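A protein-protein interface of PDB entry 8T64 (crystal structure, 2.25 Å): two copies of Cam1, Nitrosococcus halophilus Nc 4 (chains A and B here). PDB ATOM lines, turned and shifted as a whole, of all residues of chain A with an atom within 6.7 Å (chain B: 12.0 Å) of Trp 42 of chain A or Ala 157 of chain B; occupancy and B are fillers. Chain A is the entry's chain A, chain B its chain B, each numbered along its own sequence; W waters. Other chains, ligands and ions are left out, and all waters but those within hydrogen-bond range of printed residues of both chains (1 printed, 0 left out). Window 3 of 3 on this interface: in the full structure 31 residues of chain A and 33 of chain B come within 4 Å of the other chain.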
ATOM      1  N   PHE A  32     -18.549 -17.976  15.511  1.00  0.00           N
ATOM      2  CA  PHE A  32     -17.149 -17.702  15.699  1.00  0.00           C
ATOM      3  C   PHE A  32     -16.223 -18.895  15.646  1.00  0.00           C
ATOM      4  O   PHE A  32     -16.502 -19.948  16.158  1.00  0.00           O
ATOM      5  CB  PHE A  32     -16.877 -17.154  17.093  1.00  0.00           C
ATOM      6  CG  PHE A  32     -17.286 -15.760  17.319  1.00  0.00           C
ATOM      7  CD1 PHE A  32     -16.591 -14.739  16.774  1.00  0.00           C
ATOM      8  CD2 PHE A  32     -18.339 -15.487  18.128  1.00  0.00           C
ATOM      9  CE1 PHE A  32     -16.972 -13.465  16.985  1.00  0.00           C
ATOM     10  CE2 PHE A  32     -18.726 -14.216  18.354  1.00  0.00           C
ATOM     11  CZ  PHE A  32     -18.048 -13.199  17.767  1.00  0.00           C
ATOM     12  N   GLU A  37     -10.092 -15.473  23.683  1.00  0.00           N
ATOM     13  CA  GLU A  37     -11.381 -15.026  24.162  1.00  0.00           C
ATOM     14  C   GLU A  37     -11.660 -13.535  23.990  1.00  0.00           C
ATOM     15  O   GLU A  37     -12.762 -13.135  23.849  1.00  0.00           O
ATOM     16  CB  GLU A  37     -11.607 -15.491  25.590  1.00  0.00           C
ATOM     17  CG  GLU A  37     -10.897 -14.673  26.615  1.00  0.00           C
ATOM     18  CD  GLU A  37     -11.373 -14.940  28.011  1.00  0.00           C
ATOM     19  OE1 GLU A  37     -11.165 -16.023  28.558  1.00  0.00           O
ATOM     20  OE2 GLU A  37     -11.898 -14.021  28.596  1.00  0.00           O
ATOM     21  N   SER A  38     -10.629 -12.728  23.967  1.00  0.00           N
ATOM     22  CA  SER A  38     -10.776 -11.317  23.807  1.00  0.00           C
ATOM     23  C   SER A  38     -11.488 -10.836  22.585  1.00  0.00           C
ATOM     24  O   SER A  38     -12.378 -10.055  22.698  1.00  0.00           O
ATOM     25  CB  SER A  38      -9.420 -10.678  23.784  1.00  0.00           C
ATOM     26  OG  SER A  38      -8.737 -11.019  24.934  1.00  0.00           O
ATOM     27  N   VAL A  39     -11.051 -11.267  21.422  1.00  0.00           N
ATOM     28  CA  VAL A  39     -11.606 -10.794  20.166  1.00  0.00           C
ATOM     29  C   VAL A  39     -13.085 -11.047  19.947  1.00  0.00           C
ATOM     30  O   VAL A  39     -13.752 -10.179  19.482  1.00  0.00           O
ATOM     31  CB  VAL A  39     -10.774 -11.249  18.963  1.00  0.00           C
ATOM     32  CG1 VAL A  39     -11.389 -10.795  17.664  1.00  0.00           C
ATOM     33  CG2 VAL A  39      -9.401 -10.686  19.092  1.00  0.00           C
ATOM     34  N   PRO A  40     -13.572 -12.248  20.263  1.00  0.00           N
ATOM     35  CA  PRO A  40     -14.972 -12.600  20.143  1.00  0.00           C
ATOM     36  C   PRO A  40     -15.797 -11.737  21.064  1.00  0.00           C
ATOM     37  O   PRO A  40     -16.827 -11.289  20.669  1.00  0.00           O
ATOM     38  CB  PRO A  40     -14.993 -14.032  20.591  1.00  0.00           C
ATOM     39  CG  PRO A  40     -13.689 -14.531  20.203  1.00  0.00           C
ATOM     40  CD  PRO A  40     -12.743 -13.433  20.441  1.00  0.00           C
ATOM     41  N   ARG A  41     -15.310 -11.494  22.265  1.00  0.00           N
ATOM     42  CA  ARG A  41     -15.977 -10.632  23.198  1.00  0.00           C
ATOM     43  C   ARG A  41     -16.174  -9.260  22.594  1.00  0.00           C
ATOM     44  O   ARG A  41     -17.244  -8.705  22.679  1.00  0.00           O
ATOM     45  CB  ARG A  41     -15.146 -10.482  24.441  1.00  0.00           C
ATOM     46  CG  ARG A  41     -15.582 -11.304  25.619  1.00  0.00           C
ATOM     47  CD  ARG A  41     -16.868 -10.780  26.234  1.00  0.00           C
ATOM     48  NE  ARG A  41     -16.702  -9.719  27.221  1.00  0.00           N
ATOM     49  CZ  ARG A  41     -16.146  -9.867  28.404  1.00  0.00           C
ATOM     50  NH1 ARG A  41     -15.656 -11.027  28.779  1.00  0.00           N
ATOM     51  NH2 ARG A  41     -16.065  -8.839  29.210  1.00  0.00           N
ATOM     52  N   TRP A  42     -15.131  -8.720  21.982  1.00  0.00           N
ATOM     53  CA  TRP A  42     -15.189  -7.420  21.351  1.00  0.00           C
ATOM     54  C   TRP A  42     -16.228  -7.368  20.240  1.00  0.00           C
ATOM     55  O   TRP A  42     -16.935  -6.407  20.094  1.00  0.00           O
ATOM     56  CB  TRP A  42     -13.822  -7.011  20.821  1.00  0.00           C
ATOM     57  CG  TRP A  42     -13.814  -5.676  20.218  1.00  0.00           C
ATOM     58  CD1 TRP A  42     -13.615  -4.502  20.853  1.00  0.00           C
ATOM     59  CD2 TRP A  42     -14.040  -5.355  18.861  1.00  0.00           C
ATOM     60  NE1 TRP A  42     -13.700  -3.475  19.987  1.00  0.00           N
ATOM     61  CE2 TRP A  42     -13.964  -3.968  18.749  1.00  0.00           C
ATOM     62  CE3 TRP A  42     -14.295  -6.103  17.727  1.00  0.00           C
ATOM     63  CZ2 TRP A  42     -14.128  -3.316  17.560  1.00  0.00           C
ATOM     64  CZ3 TRP A  42     -14.467  -5.455  16.553  1.00  0.00           C
ATOM     65  CH2 TRP A  42     -14.379  -4.070  16.471  1.00  0.00           C
ATOM     66  N   VAL A  43     -16.314  -8.424  19.462  1.00  0.00           N
ATOM     67  CA  VAL A  43     -17.272  -8.494  18.391  1.00  0.00           C
ATOM     68  C   VAL A  43     -18.695  -8.612  18.909  1.00  0.00           C
ATOM     69  O   VAL A  43     -19.604  -8.129  18.291  1.00  0.00           O
ATOM     70  CB  VAL A  43     -16.958  -9.656  17.432  1.00  0.00           C
ATOM     71  CG1 VAL A  43     -17.960  -9.709  16.317  1.00  0.00           C
ATOM     72  CG2 VAL A  43     -15.546  -9.552  16.901  1.00  0.00           C
ATOM     73  N   MET A  44     -18.843  -9.272  20.044  1.00  0.00           N
ATOM     74  CA  MET A  44     -20.123  -9.446  20.699  1.00  0.00           C
ATOM     75  C   MET A  44     -20.678  -8.094  21.094  1.00  0.00           C
ATOM     76  O   MET A  44     -21.810  -7.815  20.868  1.00  0.00           O
ATOM     77  CB  MET A  44     -19.942 -10.246  21.957  1.00  0.00           C
ATOM     78  CG  MET A  44     -20.134 -11.719  21.852  1.00  0.00           C
ATOM     79  SD  MET A  44     -19.770 -12.445  23.442  1.00  0.00           S
ATOM     80  CE  MET A  44     -21.023 -11.699  24.428  1.00  0.00           C
ATOM     81  N   ALA A  45     -19.845  -7.265  21.690  1.00  0.00           N
ATOM     82  CA  ALA A  45     -20.226  -5.928  22.089  1.00  0.00           C
ATOM     83  C   ALA A  45     -20.591  -5.054  20.910  1.00  0.00           C
ATOM     84  O   ALA A  45     -21.461  -4.259  21.006  1.00  0.00           O
ATOM     85  CB  ALA A  45     -19.132  -5.288  22.898  1.00  0.00           C
ATOM     86  N   GLN A  46     -19.918  -5.195  19.791  1.00  0.00           N
ATOM     87  CA  GLN A  46     -20.270  -4.426  18.615  1.00  0.00           C
ATOM     88  C   GLN A  46     -21.563  -4.869  17.912  1.00  0.00           C
ATOM     89  O   GLN A  46     -22.330  -4.071  17.473  1.00  0.00           O
ATOM     90  CB  GLN A  46     -19.144  -4.510  17.608  1.00  0.00           C
ATOM     91  CG  GLN A  46     -17.819  -4.021  18.100  1.00  0.00           C
ATOM     92  CD  GLN A  46     -17.572  -2.604  17.692  1.00  0.00           C
ATOM     93  OE1 GLN A  46     -17.540  -2.266  16.513  1.00  0.00           O
ATOM     94  NE2 GLN A  46     -17.419  -1.763  18.663  1.00  0.00           N
ATOM     95  N   ILE A  47     -21.792  -6.151  17.806  1.00  0.00           N
ATOM     96  CA  ILE A  47     -22.939  -6.664  17.101  1.00  0.00           C
ATOM     97  C   ILE A  47     -24.187  -6.897  17.922  1.00  0.00           C
ATOM     98  O   ILE A  47     -25.267  -6.833  17.396  1.00  0.00           O
ATOM     99  CB  ILE A  47     -22.589  -8.017  16.471  1.00  0.00           C
ATOM    100  CG1 ILE A  47     -21.670  -7.849  15.272  1.00  0.00           C
ATOM    101  CG2 ILE A  47     -23.830  -8.821  16.152  1.00  0.00           C
ATOM    102  CD1 ILE A  47     -21.815  -6.547  14.545  1.00  0.00           C
ATOM    103  N   VAL A 141     -11.929  -9.239  11.843  1.00  0.00           N
ATOM    104  CA  VAL A 141     -11.505  -8.119  12.674  1.00  0.00           C
ATOM    105  C   VAL A 141     -10.088  -7.734  12.268  1.00  0.00           C
ATOM    106  O   VAL A 141      -9.139  -8.474  12.533  1.00  0.00           O
ATOM    107  CB  VAL A 141     -11.570  -8.465  14.166  1.00  0.00           C
ATOM    108  CG1 VAL A 141     -11.045  -7.314  14.993  1.00  0.00           C
ATOM    109  CG2 VAL A 141     -12.984  -8.813  14.552  1.00  0.00           C
ATOM    110  N   ALA A 142      -9.935  -6.573  11.634  1.00  0.00           N
ATOM    111  CA  ALA A 142      -8.623  -6.060  11.261  1.00  0.00           C
ATOM    112  C   ALA A 142      -8.087  -5.167  12.373  1.00  0.00           C
ATOM    113  O   ALA A 142      -8.773  -4.236  12.807  1.00  0.00           O
ATOM    114  CB  ALA A 142      -8.705  -5.282   9.947  1.00  0.00           C
ATOM    115  N   THR A 143      -6.867  -5.450  12.830  1.00  0.00           N
ATOM    116  CA  THR A 143      -6.263  -4.704  13.941  1.00  0.00           C
ATOM    117  C   THR A 143      -4.956  -4.009  13.558  1.00  0.00           C
ATOM    118  O   THR A 143      -4.276  -4.409  12.616  1.00  0.00           O
ATOM    119  CB  THR A 143      -5.974  -5.613  15.142  1.00  0.00           C
ATOM    120  OG1 THR A 143      -5.402  -6.844  14.679  1.00  0.00           O
ATOM    121  CG2 THR A 143      -7.251  -5.896  15.923  1.00  0.00           C
ATOM    122  N   ASN B  88      -6.140  -5.322   4.166  1.00  0.00           N
ATOM    123  CA  ASN B  88      -7.366  -5.747   4.828  1.00  0.00           C
ATOM    124  C   ASN B  88      -8.542  -5.936   3.871  1.00  0.00           C
ATOM    125  O   ASN B  88      -9.604  -6.393   4.311  1.00  0.00           O
ATOM    126  CB  ASN B  88      -7.734  -4.744   5.913  1.00  0.00           C
ATOM    127  CG  ASN B  88      -6.747  -4.751   7.049  1.00  0.00           C
ATOM    128  OD1 ASN B  88      -6.420  -5.810   7.603  1.00  0.00           O
ATOM    129  ND2 ASN B  88      -6.250  -3.569   7.403  1.00  0.00           N
ATOM    130  N   LYS B 120      -1.709 -11.477   5.882  1.00  0.00           N
ATOM    131  CA  LYS B 120      -2.840 -11.481   6.788  1.00  0.00           C
ATOM    132  C   LYS B 120      -3.978 -12.308   6.212  1.00  0.00           C
ATOM    133  O   LYS B 120      -4.019 -12.633   5.014  1.00  0.00           O
ATOM    134  CB  LYS B 120      -3.329 -10.066   7.075  1.00  0.00           C
ATOM    135  CG  LYS B 120      -3.453  -9.174   5.856  1.00  0.00           C
ATOM    136  CD  LYS B 120      -3.859  -7.784   6.325  1.00  0.00           C
ATOM    137  CE  LYS B 120      -2.849  -7.247   7.335  1.00  0.00           C
ATOM    138  NZ  LYS B 120      -2.974  -5.782   7.497  1.00  0.00           N
ATOM    139  N   MET B 154      -7.019  -3.562  20.817  1.00  0.00           N
ATOM    140  CA  MET B 154      -8.421  -3.627  20.413  1.00  0.00           C
ATOM    141  C   MET B 154      -9.012  -2.237  20.217  1.00  0.00           C
ATOM    142  O   MET B 154     -10.180  -2.097  19.856  1.00  0.00           O
ATOM    143  CB  MET B 154      -9.262  -4.403  21.437  1.00  0.00           C
ATOM    144  CG  MET B 154      -9.199  -5.929  21.301  1.00  0.00           C
ATOM    145  SD  MET B 154      -8.980  -6.510  19.604  1.00  0.00           S
ATOM    146  CE  MET B 154     -10.663  -6.631  19.015  1.00  0.00           C
ATOM    147  N   ARG B 155      -8.215  -1.199  20.466  1.00  0.00           N
ATOM    148  CA  ARG B 155      -8.654   0.141  20.096  1.00  0.00           C
ATOM    149  C   ARG B 155      -8.427   0.414  18.617  1.00  0.00           C
ATOM    150  O   ARG B 155      -9.075   1.301  18.051  1.00  0.00           O
ATOM    151  CB  ARG B 155      -7.943   1.199  20.944  1.00  0.00           C
ATOM    152  CG  ARG B 155      -6.483   0.890  21.249  1.00  0.00           C
ATOM    153  CD  ARG B 155      -6.054   1.626  22.515  1.00  0.00           C
ATOM    154  NE  ARG B 155      -6.642   2.965  22.595  1.00  0.00           N
ATOM    155  CZ  ARG B 155      -6.955   3.594  23.726  1.00  0.00           C
ATOM    156  NH1 ARG B 155      -6.748   3.020  24.905  1.00  0.00           N
ATOM    157  NH2 ARG B 155      -7.475   4.810  23.674  1.00  0.00           N
ATOM    158  N   THR B 156      -7.530  -0.339  17.984  1.00  0.00           N
ATOM    159  CA  THR B 156      -7.299  -0.250  16.551  1.00  0.00           C
ATOM    160  C   THR B 156      -8.312  -1.047  15.734  1.00  0.00           C
ATOM    161  O   THR B 156      -8.419  -0.828  14.520  1.00  0.00           O
ATOM    162  CB  THR B 156      -5.887  -0.749  16.235  1.00  0.00           C
ATOM    163  OG1 THR B 156      -5.754  -0.987  14.823  1.00  0.00           O
ATOM    164  CG2 THR B 156      -5.597  -2.043  17.009  1.00  0.00           C
ATOM    165  N   ALA B 157      -9.057  -1.950  16.363  1.00  0.00           N
ATOM    166  CA  ALA B 157      -9.805  -2.943  15.609  1.00  0.00           C
ATOM    167  C   ALA B 157     -10.977  -2.316  14.872  1.00  0.00           C
ATOM    168  O   ALA B 157     -11.708  -1.484  15.418  1.00  0.00           O
ATOM    169  CB  ALA B 157     -10.301  -4.044  16.541  1.00  0.00           C
ATOM    170  N   THR B 158     -11.160  -2.717  13.621  1.00  0.00           N
ATOM    171  CA  THR B 158     -12.408  -2.472  12.921  1.00  0.00           C
ATOM    172  C   THR B 158     -13.004  -3.809  12.516  1.00  0.00           C
ATOM    173  O   THR B 158     -12.285  -4.782  12.262  1.00  0.00           O
ATOM    174  CB  THR B 158     -12.229  -1.585  11.663  1.00  0.00           C
ATOM    175  OG1 THR B 158     -10.995  -1.900  11.004  1.00  0.00           O
ATOM    176  CG2 THR B 158     -12.256  -0.106  12.014  1.00  0.00           C
ATOM    177  N   LEU B 159     -14.323  -3.852  12.453  1.00  0.00           N
ATOM    178  CA  LEU B 159     -15.016  -4.997  11.896  1.00  0.00           C
ATOM    179  C   LEU B 159     -15.218  -4.774  10.405  1.00  0.00           C
ATOM    180  O   LEU B 159     -15.724  -3.728   9.991  1.00  0.00           O
ATOM    181  CB  LEU B 159     -16.352  -5.205  12.594  1.00  0.00           C
ATOM    182  CG  LEU B 159     -17.032  -6.516  12.244  1.00  0.00           C
ATOM    183  CD1 LEU B 159     -16.501  -7.587  13.164  1.00  0.00           C
ATOM    184  CD2 LEU B 159     -18.541  -6.365  12.391  1.00  0.00           C
ATOM    185  N   ARG B 160     -14.822  -5.738   9.601  1.00  0.00           N
ATOM    186  CA  ARG B 160     -14.902  -5.643   8.170  1.00  0.00           C
ATOM    187  C   ARG B 160     -15.611  -6.810   7.558  1.00  0.00           C
ATOM    188  O   ARG B 160     -15.705  -7.833   8.146  1.00  0.00           O
ATOM    189  CB  ARG B 160     -13.503  -5.551   7.585  1.00  0.00           C
ATOM    190  CG  ARG B 160     -12.952  -4.146   7.567  1.00  0.00           C
ATOM    191  CD  ARG B 160     -11.522  -4.106   7.100  1.00  0.00           C
ATOM    192  NE  ARG B 160     -11.128  -2.895   6.385  1.00  0.00           N
ATOM    193  CZ  ARG B 160     -11.065  -2.799   5.062  1.00  0.00           C
ATOM    194  NH1 ARG B 160     -10.664  -1.682   4.493  1.00  0.00           N
ATOM    195  NH2 ARG B 160     -11.425  -3.811   4.310  1.00  0.00           N
ATOM    196  N   GLN B 161     -16.129  -6.636   6.359  1.00  0.00           N
ATOM    197  CA  GLN B 161     -16.787  -7.714   5.670  1.00  0.00           C
ATOM    198  C   GLN B 161     -15.870  -8.311   4.639  1.00  0.00           C
ATOM    199  O   GLN B 161     -15.196  -7.626   3.934  1.00  0.00           O
ATOM    200  CB  GLN B 161     -18.091  -7.276   5.054  1.00  0.00           C
ATOM    201  CG  GLN B 161     -19.301  -7.900   5.728  1.00  0.00           C
ATOM    202  CD  GLN B 161     -20.566  -7.864   4.903  1.00  0.00           C
ATOM    203  OE1 GLN B 161     -20.634  -8.443   3.837  1.00  0.00           O
ATOM    204  NE2 GLN B 161     -21.562  -7.181   5.394  1.00  0.00           N
HETATM  205  O   HOH W   1      -8.033  -1.851  11.951  1.00  0.00           O
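The backbone carbonyl oxygen of Ala 142 of chain A lies within hydrogen-bond range of the backbone NH of Thr 158 of chain B.
Water W1 lies within hydrogen-bond range of O of Ala 142 of chain A (2.6 Å), O of Thr 156 of chain B (2.8 Å) and OG1 of Thr 158 of chain B (3.1 Å).
NH2 of Arg 160 of chain B lies within hydrogen-bond range of O of Asn 88 of chain B (3.2 Å). The side-chain amino group (NZ) of Lys 120 of chain B lies within hydrogen-bond range of the side-chain amide oxygen (OD1) of Asn 88 of chain B (3.4 Å).
Among the printed residues, pairs that only touch across the chains: Ala 142 of chain A with Ala 157 of chain B, Ala 142 of chain A with Asn 88 of chain B, Thr 143 of chain A with Thr 156 of chain B, Val 141 of chain A with Thr 158 of chain B, Trp 42 of chain A with Met 154 of chain B, Thr 143 of chain A with Ala 157 of chain B, Val 141 of chain A with Ala 157 of chain B, Trp 42 of chain A with Ala 157 of chain B, Ala 142 of chain A with Thr 156 of chain B, Ile 47 of chain A with Leu 159 of chain B and Val 141 of chain A with Leu 159 of chain B.
Of chain B, only Met 154 (3.5 Å) and Ala 157 (3.7 Å) come within 4 Å of Trp 42 of chain A. Of the printed residues of chain A, Ala 157 of chain B touches Trp 42, Val 141, Ala 142 and Thr 143. No residue of chain B comes within 4 Å of Ser 38 of chain A. No residue of chain B comes within 4 Å of Val 39 of chain A. Pro 40 of chain A touches none of the printed residues of chain B. No residue of chain B comes within 4 Å of Arg 41 of chain A. No residue of chain B comes within 4 Å of Met 44 of chain A. No residue of chain B comes within 4 Å of Gln 46 of chain A. Of chain B, only Thr 156 and Ala 157 come within 4 Å of Thr 143 of chain A. Of the printed residues of chain A, Thr 158 of chain B touches Val 141 and Ala 142. Of the printed residues of chain A, Asn 88 of chain B touches Ala 142. Gln 161 of chain B touches none of the printed residues of chain A. Arg 160 of chain B touches none of the printed residues of chain A.
Of the 15 printed residues of chain A, 5 touch a printed residue of chain B. Printed residues of chain A that touch a printed residue of chain B: Trp 42, Ile 47, Val 141, Ala 142 and Thr 143. Printed residues of chain B that touch a printed residue of chain A: Asn 88, Met 154, Thr 156, Ala 157, Thr 158 and Leu 159. Among the printed residues, 12 pairs touch across the chains. Among the printed residues, no Asp or Glu carboxylate lies within 4 Å of a Lys or Arg side-chain nitrogen of the other chain.
No position is printed for both chains.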
